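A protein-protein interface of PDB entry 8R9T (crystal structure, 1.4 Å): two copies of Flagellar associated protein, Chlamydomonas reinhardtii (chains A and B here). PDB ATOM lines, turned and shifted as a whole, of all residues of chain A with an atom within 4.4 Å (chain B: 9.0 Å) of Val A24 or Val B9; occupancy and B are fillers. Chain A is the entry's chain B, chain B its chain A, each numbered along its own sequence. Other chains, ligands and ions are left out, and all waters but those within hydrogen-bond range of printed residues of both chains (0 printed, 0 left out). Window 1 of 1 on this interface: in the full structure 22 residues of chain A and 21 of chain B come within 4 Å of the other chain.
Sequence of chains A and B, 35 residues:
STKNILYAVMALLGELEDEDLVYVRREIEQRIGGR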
ATOM      1  N   LEU A  12       2.591 -12.576  34.728  1.00  0.00           N
ATOM      2  CA  LEU A  12       3.715 -13.383  34.274  1.00  0.00           C
ATOM      3  C   LEU A  12       4.900 -12.524  33.865  1.00  0.00           C
ATOM      4  O   LEU A  12       6.046 -12.936  34.046  1.00  0.00           O
ATOM      5  CB  LEU A  12       3.260 -14.254  33.111  1.00  0.00           C
ATOM      6  CG  LEU A  12       2.236 -15.316  33.478  1.00  0.00           C
ATOM      7  CD1 LEU A  12       1.684 -15.985  32.217  1.00  0.00           C
ATOM      8  CD2 LEU A  12       2.837 -16.347  34.412  1.00  0.00           C
ATOM      9  N   LEU A  13       4.652 -11.334  33.318  1.00  0.00           N
ATOM     10  CA  LEU A  13       5.753 -10.474  32.897  1.00  0.00           C
ATOM     11  C   LEU A  13       6.700 -10.201  34.054  1.00  0.00           C
ATOM     12  O   LEU A  13       7.917 -10.095  33.860  1.00  0.00           O
ATOM     13  CB  LEU A  13       5.207  -9.158  32.347  1.00  0.00           C
ATOM     14  CG  LEU A  13       5.968  -8.450  31.236  1.00  0.00           C
ATOM     15  CD1 LEU A  13       5.897  -9.252  29.954  1.00  0.00           C
ATOM     16  CD2 LEU A  13       5.390  -7.065  31.051  1.00  0.00           C
ATOM     17  N   LEU A  16       9.547 -12.643  34.433  1.00  0.00           N
ATOM     18  CA  LEU A  16      10.532 -12.709  33.371  1.00  0.00           C
ATOM     19  C   LEU A  16      11.749 -11.868  33.713  1.00  0.00           C
ATOM     20  O   LEU A  16      11.656 -10.850  34.407  1.00  0.00           O
ATOM     21  CB  LEU A  16       9.931 -12.213  32.056  1.00  0.00           C
ATOM     22  CG  LEU A  16       8.839 -13.062  31.411  1.00  0.00           C
ATOM     23  CD1 LEU A  16       8.358 -12.367  30.140  1.00  0.00           C
ATOM     24  CD2 LEU A  16       9.362 -14.438  31.110  1.00  0.00           C
ATOM     25  N   ASP A  20      14.431 -11.538  28.709  1.00  0.00           N
ATOM     26  CA  ASP A  20      13.227 -12.087  28.108  1.00  0.00           C
ATOM     27  C   ASP A  20      12.339 -10.999  27.538  1.00  0.00           C
ATOM     28  O   ASP A  20      11.637 -11.228  26.545  1.00  0.00           O
ATOM     29  CB  ASP A  20      12.440 -12.849  29.165  1.00  0.00           C
ATOM     30  CG  ASP A  20      13.207 -14.000  29.733  1.00  0.00           C
ATOM     31  OD1 ASP A  20      13.854 -14.713  28.945  1.00  0.00           O
ATOM     32  OD2 ASP A  20      13.165 -14.171  30.973  1.00  0.00           O
ATOM     33  N   LEU A  21      12.351  -9.816  28.161  1.00  0.00           N
ATOM     34  CA  LEU A  21      11.494  -8.731  27.711  1.00  0.00           C
ATOM     35  C   LEU A  21      11.857  -8.277  26.306  1.00  0.00           C
ATOM     36  O   LEU A  21      10.997  -7.748  25.590  1.00  0.00           O
ATOM     37  CB  LEU A  21      11.574  -7.569  28.695  1.00  0.00           C
ATOM     38  CG  LEU A  21      11.173  -7.881  30.135  1.00  0.00           C
ATOM     39  CD1 LEU A  21      11.304  -6.616  30.994  1.00  0.00           C
ATOM     40  CD2 LEU A  21       9.781  -8.453  30.214  1.00  0.00           C
ATOM     41  N   VAL A  22      13.117  -8.459  25.902  1.00  0.00           N
ATOM     42  CA  VAL A  22      13.525  -8.143  24.534  1.00  0.00           C
ATOM     43  C   VAL A  22      12.650  -8.882  23.529  1.00  0.00           C
ATOM     44  O   VAL A  22      12.219  -8.318  22.513  1.00  0.00           O
ATOM     45  CB  VAL A  22      15.008  -8.509  24.327  1.00  0.00           C
ATOM     46  CG1 VAL A  22      15.328  -8.552  22.825  1.00  0.00           C
ATOM     47  CG2 VAL A  22      15.916  -7.544  25.051  1.00  0.00           C
ATOM     48  N   TYR A  23      12.404 -10.166  23.781  1.00  0.00           N
ATOM     49  CA  TYR A  23      11.642 -10.975  22.843  1.00  0.00           C
ATOM     50  C   TYR A  23      10.173 -10.603  22.869  1.00  0.00           C
ATOM     51  O   TYR A  23       9.529 -10.554  21.819  1.00  0.00           O
ATOM     52  CB  TYR A  23      11.861 -12.455  23.147  1.00  0.00           C
ATOM     53  CG  TYR A  23      13.328 -12.800  23.020  1.00  0.00           C
ATOM     54  CD1 TYR A  23      13.925 -12.855  21.773  1.00  0.00           C
ATOM     55  CD2 TYR A  23      14.125 -13.000  24.138  1.00  0.00           C
ATOM     56  CE1 TYR A  23      15.248 -13.128  21.630  1.00  0.00           C
ATOM     57  CE2 TYR A  23      15.466 -13.274  24.007  1.00  0.00           C
ATOM     58  CZ  TYR A  23      16.023 -13.341  22.742  1.00  0.00           C
ATOM     59  OH  TYR A  23      17.362 -13.601  22.559  1.00  0.00           O
ATOM     60  N   VAL A  24       9.635 -10.308  24.053  1.00  0.00           N
ATOM     61  CA  VAL A  24       8.260  -9.828  24.138  1.00  0.00           C
ATOM     62  C   VAL A  24       8.114  -8.514  23.379  1.00  0.00           C
ATOM     63  O   VAL A  24       7.165  -8.319  22.607  1.00  0.00           O
ATOM     64  CB  VAL A  24       7.820  -9.698  25.607  1.00  0.00           C
ATOM     65  CG1 VAL A  24       6.369  -9.238  25.668  1.00  0.00           C
ATOM     66  CG2 VAL A  24       7.990 -11.028  26.329  1.00  0.00           C
ATOM     67  N   ARG A  25       9.046  -7.590  23.611  1.00  0.00           N
ATOM     68  CA  ARG A  25       8.999  -6.295  22.939  1.00  0.00           C
ATOM     69  C   ARG A  25       9.061  -6.472  21.427  1.00  0.00           C
ATOM     70  O   ARG A  25       8.357  -5.778  20.685  1.00  0.00           O
ATOM     71  CB  ARG A  25      10.160  -5.426  23.432  1.00  0.00           C
ATOM     72  CG  ARG A  25      10.133  -3.975  22.950  1.00  0.00           C
ATOM     73  CD  ARG A  25      11.285  -3.152  23.574  1.00  0.00           C
ATOM     74  NE  ARG A  25      12.610  -3.657  23.225  1.00  0.00           N
ATOM     75  CZ  ARG A  25      13.732  -3.291  23.834  1.00  0.00           C
ATOM     76  NH1 ARG A  25      13.694  -2.415  24.830  1.00  0.00           N
ATOM     77  NH2 ARG A  25      14.894  -3.803  23.447  1.00  0.00           N
ATOM     78  N   ARG A  26       9.892  -7.398  20.956  1.00  0.00           N
ATOM     79  CA  ARG A  26      10.007  -7.610  19.521  1.00  0.00           C
ATOM     80  C   ARG A  26       8.689  -8.105  18.941  1.00  0.00           C
ATOM     81  O   ARG A  26       8.268  -7.657  17.868  1.00  0.00           O
ATOM     82  CB  ARG A  26      11.129  -8.598  19.233  1.00  0.00           C
ATOM     83  CG  ARG A  26      11.590  -8.555  17.802  1.00  0.00           C
ATOM     84  CD  ARG A  26      12.955  -9.185  17.659  1.00  0.00           C
ATOM     85  NE  ARG A  26      12.942 -10.576  18.077  1.00  0.00           N
ATOM     86  CZ  ARG A  26      14.001 -11.384  18.015  1.00  0.00           C
ATOM     87  NH1 ARG A  26      15.159 -10.924  17.583  1.00  0.00           N
ATOM     88  NH2 ARG A  26      13.907 -12.645  18.399  1.00  0.00           N
ATOM     89  N   GLU A  27       8.010  -9.016  19.646  1.00  0.00           N
ATOM     90  CA  GLU A  27       6.730  -9.510  19.155  1.00  0.00           C
ATOM     91  C   GLU A  27       5.708  -8.382  19.080  1.00  0.00           C
ATOM     92  O   GLU A  27       4.940  -8.292  18.112  1.00  0.00           O
ATOM     93  CB  GLU A  27       6.231 -10.648  20.046  1.00  0.00           C
ATOM     94  CG  GLU A  27       4.951 -11.314  19.565  1.00  0.00           C
ATOM     95  CD  GLU A  27       5.019 -11.759  18.105  1.00  0.00           C
ATOM     96  OE1 GLU A  27       6.073 -12.292  17.670  1.00  0.00           O
ATOM     97  OE2 GLU A  27       4.009 -11.575  17.388  1.00  0.00           O
ATOM     98  N   ILE A  28       5.699  -7.502  20.085  1.00  0.00           N
ATOM     99  CA  ILE A  28       4.800  -6.353  20.081  1.00  0.00           C
ATOM    100  C   ILE A  28       5.123  -5.419  18.924  1.00  0.00           C
ATOM    101  O   ILE A  28       4.222  -4.948  18.222  1.00  0.00           O
ATOM    102  CB  ILE A  28       4.869  -5.621  21.436  1.00  0.00           C
ATOM    103  CG1 ILE A  28       4.303  -6.523  22.532  1.00  0.00           C
ATOM    104  CG2 ILE A  28       4.160  -4.287  21.361  1.00  0.00           C
ATOM    105  CD1 ILE A  28       4.553  -6.024  23.926  1.00  0.00           C
ATOM    106  N   THR B   2      13.920 -19.085  32.672  1.00  0.00           N
ATOM    107  CA  THR B   2      12.591 -18.495  32.557  1.00  0.00           C
ATOM    108  C   THR B   2      11.866 -18.942  31.296  1.00  0.00           C
ATOM    109  O   THR B   2      10.857 -18.335  30.930  1.00  0.00           O
ATOM    110  CB  THR B   2      12.717 -16.975  32.542  1.00  0.00           C
ATOM    111  OG1 THR B   2      13.679 -16.624  31.535  1.00  0.00           O
ATOM    112  CG2 THR B   2      13.165 -16.456  33.901  1.00  0.00           C
ATOM    113  N   LYS B   3      12.336 -20.003  30.638  1.00  0.00           N
ATOM    114  CA  LYS B   3      11.811 -20.348  29.324  1.00  0.00           C
ATOM    115  C   LYS B   3      10.346 -20.761  29.369  1.00  0.00           C
ATOM    116  O   LYS B   3       9.610 -20.492  28.416  1.00  0.00           O
ATOM    117  CB  LYS B   3      12.671 -21.428  28.683  1.00  0.00           C
ATOM    118  CG  LYS B   3      13.967 -20.882  28.084  1.00  0.00           C
ATOM    119  CD  LYS B   3      14.845 -21.988  27.541  1.00  0.00           C
ATOM    120  CE  LYS B   3      16.064 -21.407  26.821  1.00  0.00           C
ATOM    121  NZ  LYS B   3      17.020 -22.471  26.437  1.00  0.00           N
ATOM    122  N   ASN B   4       9.887 -21.400  30.452  1.00  0.00           N
ATOM    123  CA  ASN B   4       8.467 -21.747  30.496  1.00  0.00           C
ATOM    124  C   ASN B   4       7.610 -20.493  30.544  1.00  0.00           C
ATOM    125  O   ASN B   4       6.548 -20.427  29.910  1.00  0.00           O
ATOM    126  CB  ASN B   4       8.119 -22.587  31.726  1.00  0.00           C
ATOM    127  CG  ASN B   4       8.556 -24.017  31.612  1.00  0.00           C
ATOM    128  OD1 ASN B   4       8.553 -24.605  30.532  1.00  0.00           O
ATOM    129  ND2 ASN B   4       8.899 -24.609  32.749  1.00  0.00           N
ATOM    130  N   ILE B   5       8.039 -19.506  31.324  1.00  0.00           N
ATOM    131  CA  ILE B   5       7.263 -18.284  31.456  1.00  0.00           C
ATOM    132  C   ILE B   5       7.293 -17.493  30.153  1.00  0.00           C
ATOM    133  O   ILE B   5       6.265 -16.967  29.701  1.00  0.00           O
ATOM    134  CB  ILE B   5       7.746 -17.461  32.666  1.00  0.00           C
ATOM    135  CG1 ILE B   5       7.753 -18.342  33.916  1.00  0.00           C
ATOM    136  CG2 ILE B   5       6.869 -16.243  32.821  1.00  0.00           C
ATOM    137  CD1 ILE B   5       6.439 -18.422  34.632  1.00  0.00           C
ATOM    138  N   LEU B   6       8.464 -17.395  29.530  1.00  0.00           N
ATOM    139  CA  LEU B   6       8.560 -16.674  28.267  1.00  0.00           C
ATOM    140  C   LEU B   6       7.691 -17.334  27.207  1.00  0.00           C
ATOM    141  O   LEU B   6       6.957 -16.653  26.487  1.00  0.00           O
ATOM    142  CB  LEU B   6      10.017 -16.602  27.824  1.00  0.00           C
ATOM    143  CG  LEU B   6      10.272 -15.916  26.483  1.00  0.00           C
ATOM    144  CD1 LEU B   6       9.788 -14.478  26.490  1.00  0.00           C
ATOM    145  CD2 LEU B   6      11.735 -16.008  26.140  1.00  0.00           C
ATOM    146  N   TYR B   7       7.715 -18.663  27.139  1.00  0.00           N
ATOM    147  CA  TYR B   7       6.868 -19.363  26.182  1.00  0.00           C
ATOM    148  C   TYR B   7       5.407 -19.015  26.409  1.00  0.00           C
ATOM    149  O   TYR B   7       4.671 -18.709  25.459  1.00  0.00           O
ATOM    150  CB  TYR B   7       7.077 -20.865  26.319  1.00  0.00           C
ATOM    151  CG  TYR B   7       6.057 -21.691  25.570  1.00  0.00           C
ATOM    152  CD1 TYR B   7       6.149 -21.879  24.195  1.00  0.00           C
ATOM    153  CD2 TYR B   7       4.980 -22.261  26.244  1.00  0.00           C
ATOM    154  CE1 TYR B   7       5.203 -22.628  23.514  1.00  0.00           C
ATOM    155  CE2 TYR B   7       4.057 -23.022  25.580  1.00  0.00           C
ATOM    156  CZ  TYR B   7       4.152 -23.187  24.215  1.00  0.00           C
ATOM    157  OH  TYR B   7       3.170 -23.914  23.580  1.00  0.00           O
ATOM    158  N   ALA B   8       4.956 -19.086  27.662  1.00  0.00           N
ATOM    159  CA  ALA B   8       3.554 -18.807  27.960  1.00  0.00           C
ATOM    160  C   ALA B   8       3.188 -17.377  27.579  1.00  0.00           C
ATOM    161  O   ALA B   8       2.148 -17.132  26.966  1.00  0.00           O
ATOM    162  CB  ALA B   8       3.268 -19.073  29.430  1.00  0.00           C
ATOM    163  N   VAL B   9       4.038 -16.419  27.940  1.00  0.00           N
ATOM    164  CA  VAL B   9       3.741 -15.031  27.599  1.00  0.00           C
ATOM    165  C   VAL B   9       3.648 -14.851  26.098  1.00  0.00           C
ATOM    166  O   VAL B   9       2.714 -14.217  25.590  1.00  0.00           O
ATOM    167  CB  VAL B   9       4.785 -14.086  28.230  1.00  0.00           C
ATOM    168  CG1 VAL B   9       4.669 -12.700  27.615  1.00  0.00           C
ATOM    169  CG2 VAL B   9       4.583 -14.026  29.747  1.00  0.00           C
ATOM    170  N   MET B  10       4.631 -15.373  25.352  1.00  0.00           N
ATOM    171  CA  MET B  10       4.631 -15.231  23.906  1.00  0.00           C
ATOM    172  C   MET B  10       3.392 -15.866  23.293  1.00  0.00           C
ATOM    173  O   MET B  10       2.792 -15.313  22.365  1.00  0.00           O
ATOM    174  CB  MET B  10       5.895 -15.867  23.335  1.00  0.00           C
ATOM    175  CG  MET B  10       7.168 -15.209  23.827  1.00  0.00           C
ATOM    176  SD  MET B  10       7.398 -13.523  23.193  1.00  0.00           S
ATOM    177  CE  MET B  10       7.950 -13.818  21.561  1.00  0.00           C
ATOM    178  N   ALA B  11       2.974 -17.010  23.826  1.00  0.00           N
ATOM    179  CA  ALA B  11       1.784 -17.669  23.315  1.00  0.00           C
ATOM    180  C   ALA B  11       0.555 -16.811  23.563  1.00  0.00           C
ATOM    181  O   ALA B  11      -0.313 -16.688  22.691  1.00  0.00           O
ATOM    182  CB  ALA B  11       1.617 -19.034  23.979  1.00  0.00           C
ATOM    183  N   LEU B  12       0.464 -16.216  24.756  1.00  0.00           N
ATOM    184  CA  LEU B  12      -0.731 -15.485  25.137  1.00  0.00           C
ATOM    185  C   LEU B  12      -0.840 -14.140  24.442  1.00  0.00           C
ATOM    186  O   LEU B  12      -1.947 -13.614  24.311  1.00  0.00           O
ATOM    187  CB  LEU B  12      -0.754 -15.286  26.650  1.00  0.00           C
ATOM    188  CG  LEU B  12      -0.924 -16.575  27.451  1.00  0.00           C
ATOM    189  CD1 LEU B  12      -0.701 -16.335  28.942  1.00  0.00           C
ATOM    190  CD2 LEU B  12      -2.295 -17.193  27.226  1.00  0.00           C
ATOM    191  N   LEU B  13       0.270 -13.568  23.978  1.00  0.00           N
ATOM    192  CA  LEU B  13       0.150 -12.322  23.234  1.00  0.00           C
ATOM    193  C   LEU B  13      -0.714 -12.499  21.994  1.00  0.00           C
ATOM    194  O   LEU B  13      -1.359 -11.548  21.547  1.00  0.00           O
ATOM    195  CB  LEU B  13       1.518 -11.817  22.797  1.00  0.00           C
ATOM    196  CG  LEU B  13       2.544 -11.441  23.858  1.00  0.00           C
ATOM    197  CD1 LEU B  13       3.797 -10.898  23.196  1.00  0.00           C
ATOM    198  CD2 LEU B  13       1.963 -10.412  24.802  1.00  0.00           C
ATOM    199  N   GLY B  14      -0.754 -13.712  21.442  1.00  0.00           N
ATOM    200  CA  GLY B  14      -1.593 -14.002  20.298  1.00  0.00           C
ATOM    201  C   GLY B  14      -3.066 -14.021  20.607  1.00  0.00           C
ATOM    202  O   GLY B  14      -3.875 -14.056  19.671  1.00  0.00           O
ATOM    203  N   GLU B  15      -3.437 -13.981  21.882  1.00  0.00           N
ATOM    204  CA  GLU B  15      -4.832 -13.910  22.278  1.00  0.00           C
ATOM    205  C   GLU B  15      -5.259 -12.484  22.599  1.00  0.00           C
ATOM    206  O   GLU B  15      -6.409 -12.262  22.994  1.00  0.00           O
ATOM    207  CB  GLU B  15      -5.076 -14.790  23.507  1.00  0.00           C
ATOM    208  CG  GLU B  15      -4.615 -16.217  23.358  1.00  0.00           C
ATOM    209  CD  GLU B  15      -5.456 -17.009  22.378  1.00  0.00           C
ATOM    210  OE1 GLU B  15      -6.621 -16.625  22.124  1.00  0.00           O
ATOM    211  OE2 GLU B  15      -4.956 -18.033  21.873  1.00  0.00           O
ATOM    212  N   LEU B  16      -4.357 -11.517  22.454  1.00  0.00           N
ATOM    213  CA  LEU B  16      -4.640 -10.134  22.794  1.00  0.00           C
ATOM    214  C   LEU B  16      -4.773  -9.286  21.540  1.00  0.00           C
ATOM    215  O   LEU B  16      -4.131  -9.546  20.522  1.00  0.00           O
ATOM    216  CB  LEU B  16      -3.516  -9.537  23.644  1.00  0.00           C
ATOM    217  CG  LEU B  16      -3.319 -10.145  25.029  1.00  0.00           C
ATOM    218  CD1 LEU B  16      -2.158  -9.475  25.752  1.00  0.00           C
ATOM    219  CD2 LEU B  16      -4.590 -10.008  25.844  1.00  0.00           C
ATOM    220  N   LEU B  21      -1.698  -4.712  23.585  1.00  0.00           N
ATOM    221  CA  LEU B  21      -0.243  -4.797  23.625  1.00  0.00           C
ATOM    222  C   LEU B  21       0.404  -3.506  24.116  1.00  0.00           C
ATOM    223  O   LEU B  21       1.537  -3.542  24.618  1.00  0.00           O
ATOM    224  CB  LEU B  21       0.273  -5.158  22.234  1.00  0.00           C
ATOM    225  CG  LEU B  21      -0.248  -6.473  21.654  1.00  0.00           C
ATOM    226  CD1 LEU B  21       0.316  -6.639  20.240  1.00  0.00           C
ATOM    227  CD2 LEU B  21       0.100  -7.638  22.564  1.00  0.00           C
ATOM    228  N   TYR B  23      -0.319  -1.839  26.712  1.00  0.00           N
ATOM    229  CA  TYR B  23      -0.109  -1.938  28.153  1.00  0.00           C
ATOM    230  C   TYR B  23       1.086  -2.821  28.475  1.00  0.00           C
ATOM    231  O   TYR B  23       1.860  -2.515  29.393  1.00  0.00           O
ATOM    232  CB  TYR B  23      -1.372  -2.456  28.832  1.00  0.00           C
ATOM    233  CG  TYR B  23      -2.565  -1.606  28.491  1.00  0.00           C
ATOM    234  CD1 TYR B  23      -2.668  -0.309  28.969  1.00  0.00           C
ATOM    235  CD2 TYR B  23      -3.561  -2.076  27.645  1.00  0.00           C
ATOM    236  CE1 TYR B  23      -3.737   0.481  28.640  1.00  0.00           C
ATOM    237  CE2 TYR B  23      -4.642  -1.295  27.312  1.00  0.00           C
ATOM    238  CZ  TYR B  23      -4.721  -0.012  27.808  1.00  0.00           C
ATOM    239  OH  TYR B  23      -5.799   0.753  27.464  1.00  0.00           O
ATOM    240  N   VAL B  24       1.245  -3.922  27.742  1.00  0.00           N
ATOM    241  CA  VAL B  24       2.419  -4.770  27.924  1.00  0.00           C
ATOM    242  C   VAL B  24       3.678  -3.971  27.628  1.00  0.00           C
ATOM    243  O   VAL B  24       4.659  -4.024  28.379  1.00  0.00           O
ATOM    244  CB  VAL B  24       2.315  -6.038  27.059  1.00  0.00           C
ATOM    245  CG1 VAL B  24       3.500  -6.935  27.328  1.00  0.00           C
ATOM    246  CG2 VAL B  24       1.029  -6.776  27.368  1.00  0.00           C
ATOM    247  N   ARG B  25       3.658  -3.190  26.547  1.00  0.00           N
ATOM    248  CA  ARG B  25       4.821  -2.379  26.197  1.00  0.00           C
ATOM    249  C   ARG B  25       5.169  -1.401  27.316  1.00  0.00           C
ATOM    250  O   ARG B  25       6.348  -1.222  27.644  1.00  0.00           O
ATOM    251  CB  ARG B  25       4.553  -1.629  24.898  1.00  0.00           C
ATOM    252  CG  ARG B  25       5.716  -0.742  24.441  1.00  0.00           C
ATOM    253  CD  ARG B  25       5.490  -0.201  23.035  1.00  0.00           C
ATOM    254  NE  ARG B  25       4.351   0.716  22.963  1.00  0.00           N
ATOM    255  CZ  ARG B  25       3.735   1.056  21.832  1.00  0.00           C
ATOM    256  NH1 ARG B  25       4.154   0.557  20.678  1.00  0.00           N
ATOM    257  NH2 ARG B  25       2.703   1.896  21.850  1.00  0.00           N
ATOM    258  N   GLU B  27       4.674  -1.727  30.536  1.00  0.00           N
ATOM    259  CA  GLU B  27       5.318  -2.448  31.628  1.00  0.00           C
ATOM    260  C   GLU B  27       6.761  -2.800  31.281  1.00  0.00           C
ATOM    261  O   GLU B  27       7.637  -2.793  32.152  1.00  0.00           O
ATOM    262  CB  GLU B  27       4.493  -3.683  31.981  1.00  0.00           C
ATOM    263  CG  GLU B  27       3.148  -3.341  32.612  1.00  0.00           C
ATOM    264  CD  GLU B  27       3.305  -2.491  33.859  1.00  0.00           C
ATOM    265  OE1 GLU B  27       4.020  -2.931  34.778  1.00  0.00           O
ATOM    266  OE2 GLU B  27       2.728  -1.385  33.933  1.00  0.00           O
ATOM    267  N   ILE B  28       7.030  -3.123  30.012  1.00  0.00           N
ATOM    268  CA  ILE B  28       8.407  -3.372  29.600  1.00  0.00           C
ATOM    269  C   ILE B  28       9.237  -2.100  29.726  1.00  0.00           C
ATOM    270  O   ILE B  28      10.342  -2.108  30.286  1.00  0.00           O
ATOM    271  CB  ILE B  28       8.444  -3.933  28.167  1.00  0.00           C
ATOM    272  CG1 ILE B  28       7.894  -5.362  28.147  1.00  0.00           C
ATOM    273  CG2 ILE B  28       9.869  -3.879  27.628  1.00  0.00           C
ATOM    274  CD1 ILE B  28       7.637  -5.899  26.757  1.00  0.00           C
ATOM    275  N   ARG B  31      10.533  -1.071  33.070  1.00  0.00           N
ATOM    276  CA  ARG B  31      11.658  -1.820  33.609  1.00  0.00           C
ATOM    277  C   ARG B  31      12.963  -1.594  32.868  1.00  0.00           C
ATOM    278  O   ARG B  31      14.011  -1.491  33.509  1.00  0.00           O
ATOM    279  CB  ARG B  31      11.318  -3.306  33.633  1.00  0.00           C
ATOM    280  CG  ARG B  31      10.414  -3.675  34.799  1.00  0.00           C
ATOM    281  CD  ARG B  31       9.929  -5.093  34.691  1.00  0.00           C
ATOM    282  NE  ARG B  31      11.052  -6.012  34.617  1.00  0.00           N
ATOM    283  CZ  ARG B  31      10.939  -7.323  34.478  1.00  0.00           C
ATOM    284  NH1 ARG B  31       9.738  -7.889  34.412  1.00  0.00           N
ATOM    285  NH2 ARG B  31      12.041  -8.058  34.405  1.00  0.00           N
ATOM    286  N   ILE B  32      12.946  -1.529  31.538  1.00  0.00           N
ATOM    287  CA  ILE B  32      14.175  -1.446  30.763  1.00  0.00           C
ATOM    288  C   ILE B  32      14.302  -0.157  29.968  1.00  0.00           C
ATOM    289  O   ILE B  32      15.292   0.019  29.255  1.00  0.00           O
ATOM    290  CB  ILE B  32      14.379  -2.675  29.851  1.00  0.00           C
ATOM    291  CG1 ILE B  32      13.223  -2.831  28.863  1.00  0.00           C
ATOM    292  CG2 ILE B  32      14.534  -3.931  30.689  1.00  0.00           C
ATOM    293  CD1 ILE B  32      13.510  -3.886  27.787  1.00  0.00           C
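Of chain B, only Leu B6, Val B9, Met B10, Leu B13 and Ile B28 come within 4 Å of Val A24.
Val B9 touches just these residues of chain A: Leu A12 and Val A24.
Of the printed residues of chain A, Val B24 touches Ile A28.
Printed residues of chain B within 4 Å of Leu A13: Glu B27 and Arg B31.
Of the printed residues of chain B, Glu A27 touches Met B10 and Leu B13.
Of the printed residues of chain B, Asp A20 touches Thr B2 (2.6 Å) and Leu B6 (3.7 Å).
The nearest residue of chain B that does not touch Val A24 is Val B24 (4.04 Å).
The nearest residue of chain A that does not touch Val B9 is Leu A16 (4.1 Å).
The nearest printed residue of chain A that does not touch Thr B2 is Leu A16 (4.2 Å).
Leu A13 touches Glu B27, and with the chains exchanged Glu A27 touches Leu B13.
Val A24 touches Leu B13, but with the chains exchanged Leu A13 does not touch Val B24 (4.1 Å).
Arg A25 touches Ile B28, and with the chains exchanged Ile A28 touches Arg B25.
Ile A28 touches Leu B21, but with the chains exchanged Leu A21 does not touch Ile B28 (4.01 Å).
Positions printed for both chains: 12, 13, 16, 21, 23, 24, 25, 27 and 28.
Of the 23 pairs that touch across the chains among the printed residues, 6 have their exchanged pair printed and touching as well.
CG2 of Ile B5 touches O of Leu A12, 3.6 Å away.
Val B9 touches Leu A12.
Leu A13 touches Glu B27 (CD2 to CB, 3.6 Å).
Ile B5 touches Leu A16 (CG2 to CD2, 3.5 Å).
Leu B6 touches Leu A16.
Met B10 touches Tyr A23.
CG2 of Val A24 touches CD1 of Leu B6 (3.9 Å).
Leu B13 touches Val A24.
Ile B32 touches Arg A25.
Glu A27 touches Met B10.
Of the 12 printed residues of chain A, 10 touch a printed residue of chain B.
Printed residues of chain A that touch a printed residue of chain B: Leu A12, Leu A13, Leu A16, Asp A20, Leu A21, Tyr A23, Val A24, Arg A25, Glu A27 and Ile A28.
Hydrophobic or aromatic side chains of chain A within 4 Å of the printed part of chain B: Leu A12, Leu A13, Leu A16, Leu A21, Val A24 and Ile A28.
Of the 23 printed residues of chain B, 13 touch a printed residue of chain A.
Printed residues of chain B that touch a printed residue of chain A: Thr B2, Ile B5, Leu B6, Val B9, Met B10, Leu B13, Leu B21, Val B24, Arg B25, Glu B27, Ile B28, Arg B31 and Ile B32.
Hydrophobic or aromatic side chains of chain B that line the printed part of chain A: Ile B5, Leu B6, Val B9, Met B10, Leu B13, Val B24, Ile B28 and Ile B32.
Among the printed residues, no Asp or Glu carboxylate lies within 4 Å of a Lys or Arg side-chain nitrogen of the other chain.
The backbone carbonyl oxygen (O) of Leu A13 sits at hydrogen-bond distance from the guanidinium group (NH1) of Arg B31 (2.9 Å).
The side-chain hydroxyl (OG1) of Thr B2 sits at hydrogen-bond distance from the side-chain carboxylate (OD2) of Asp A20 (2.6 Å).
The backbone carbonyl oxygen (O) of Leu A16 sits at hydrogen-bond distance from the guanidinium group (NH2) of Arg B31 (2.8 Å).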
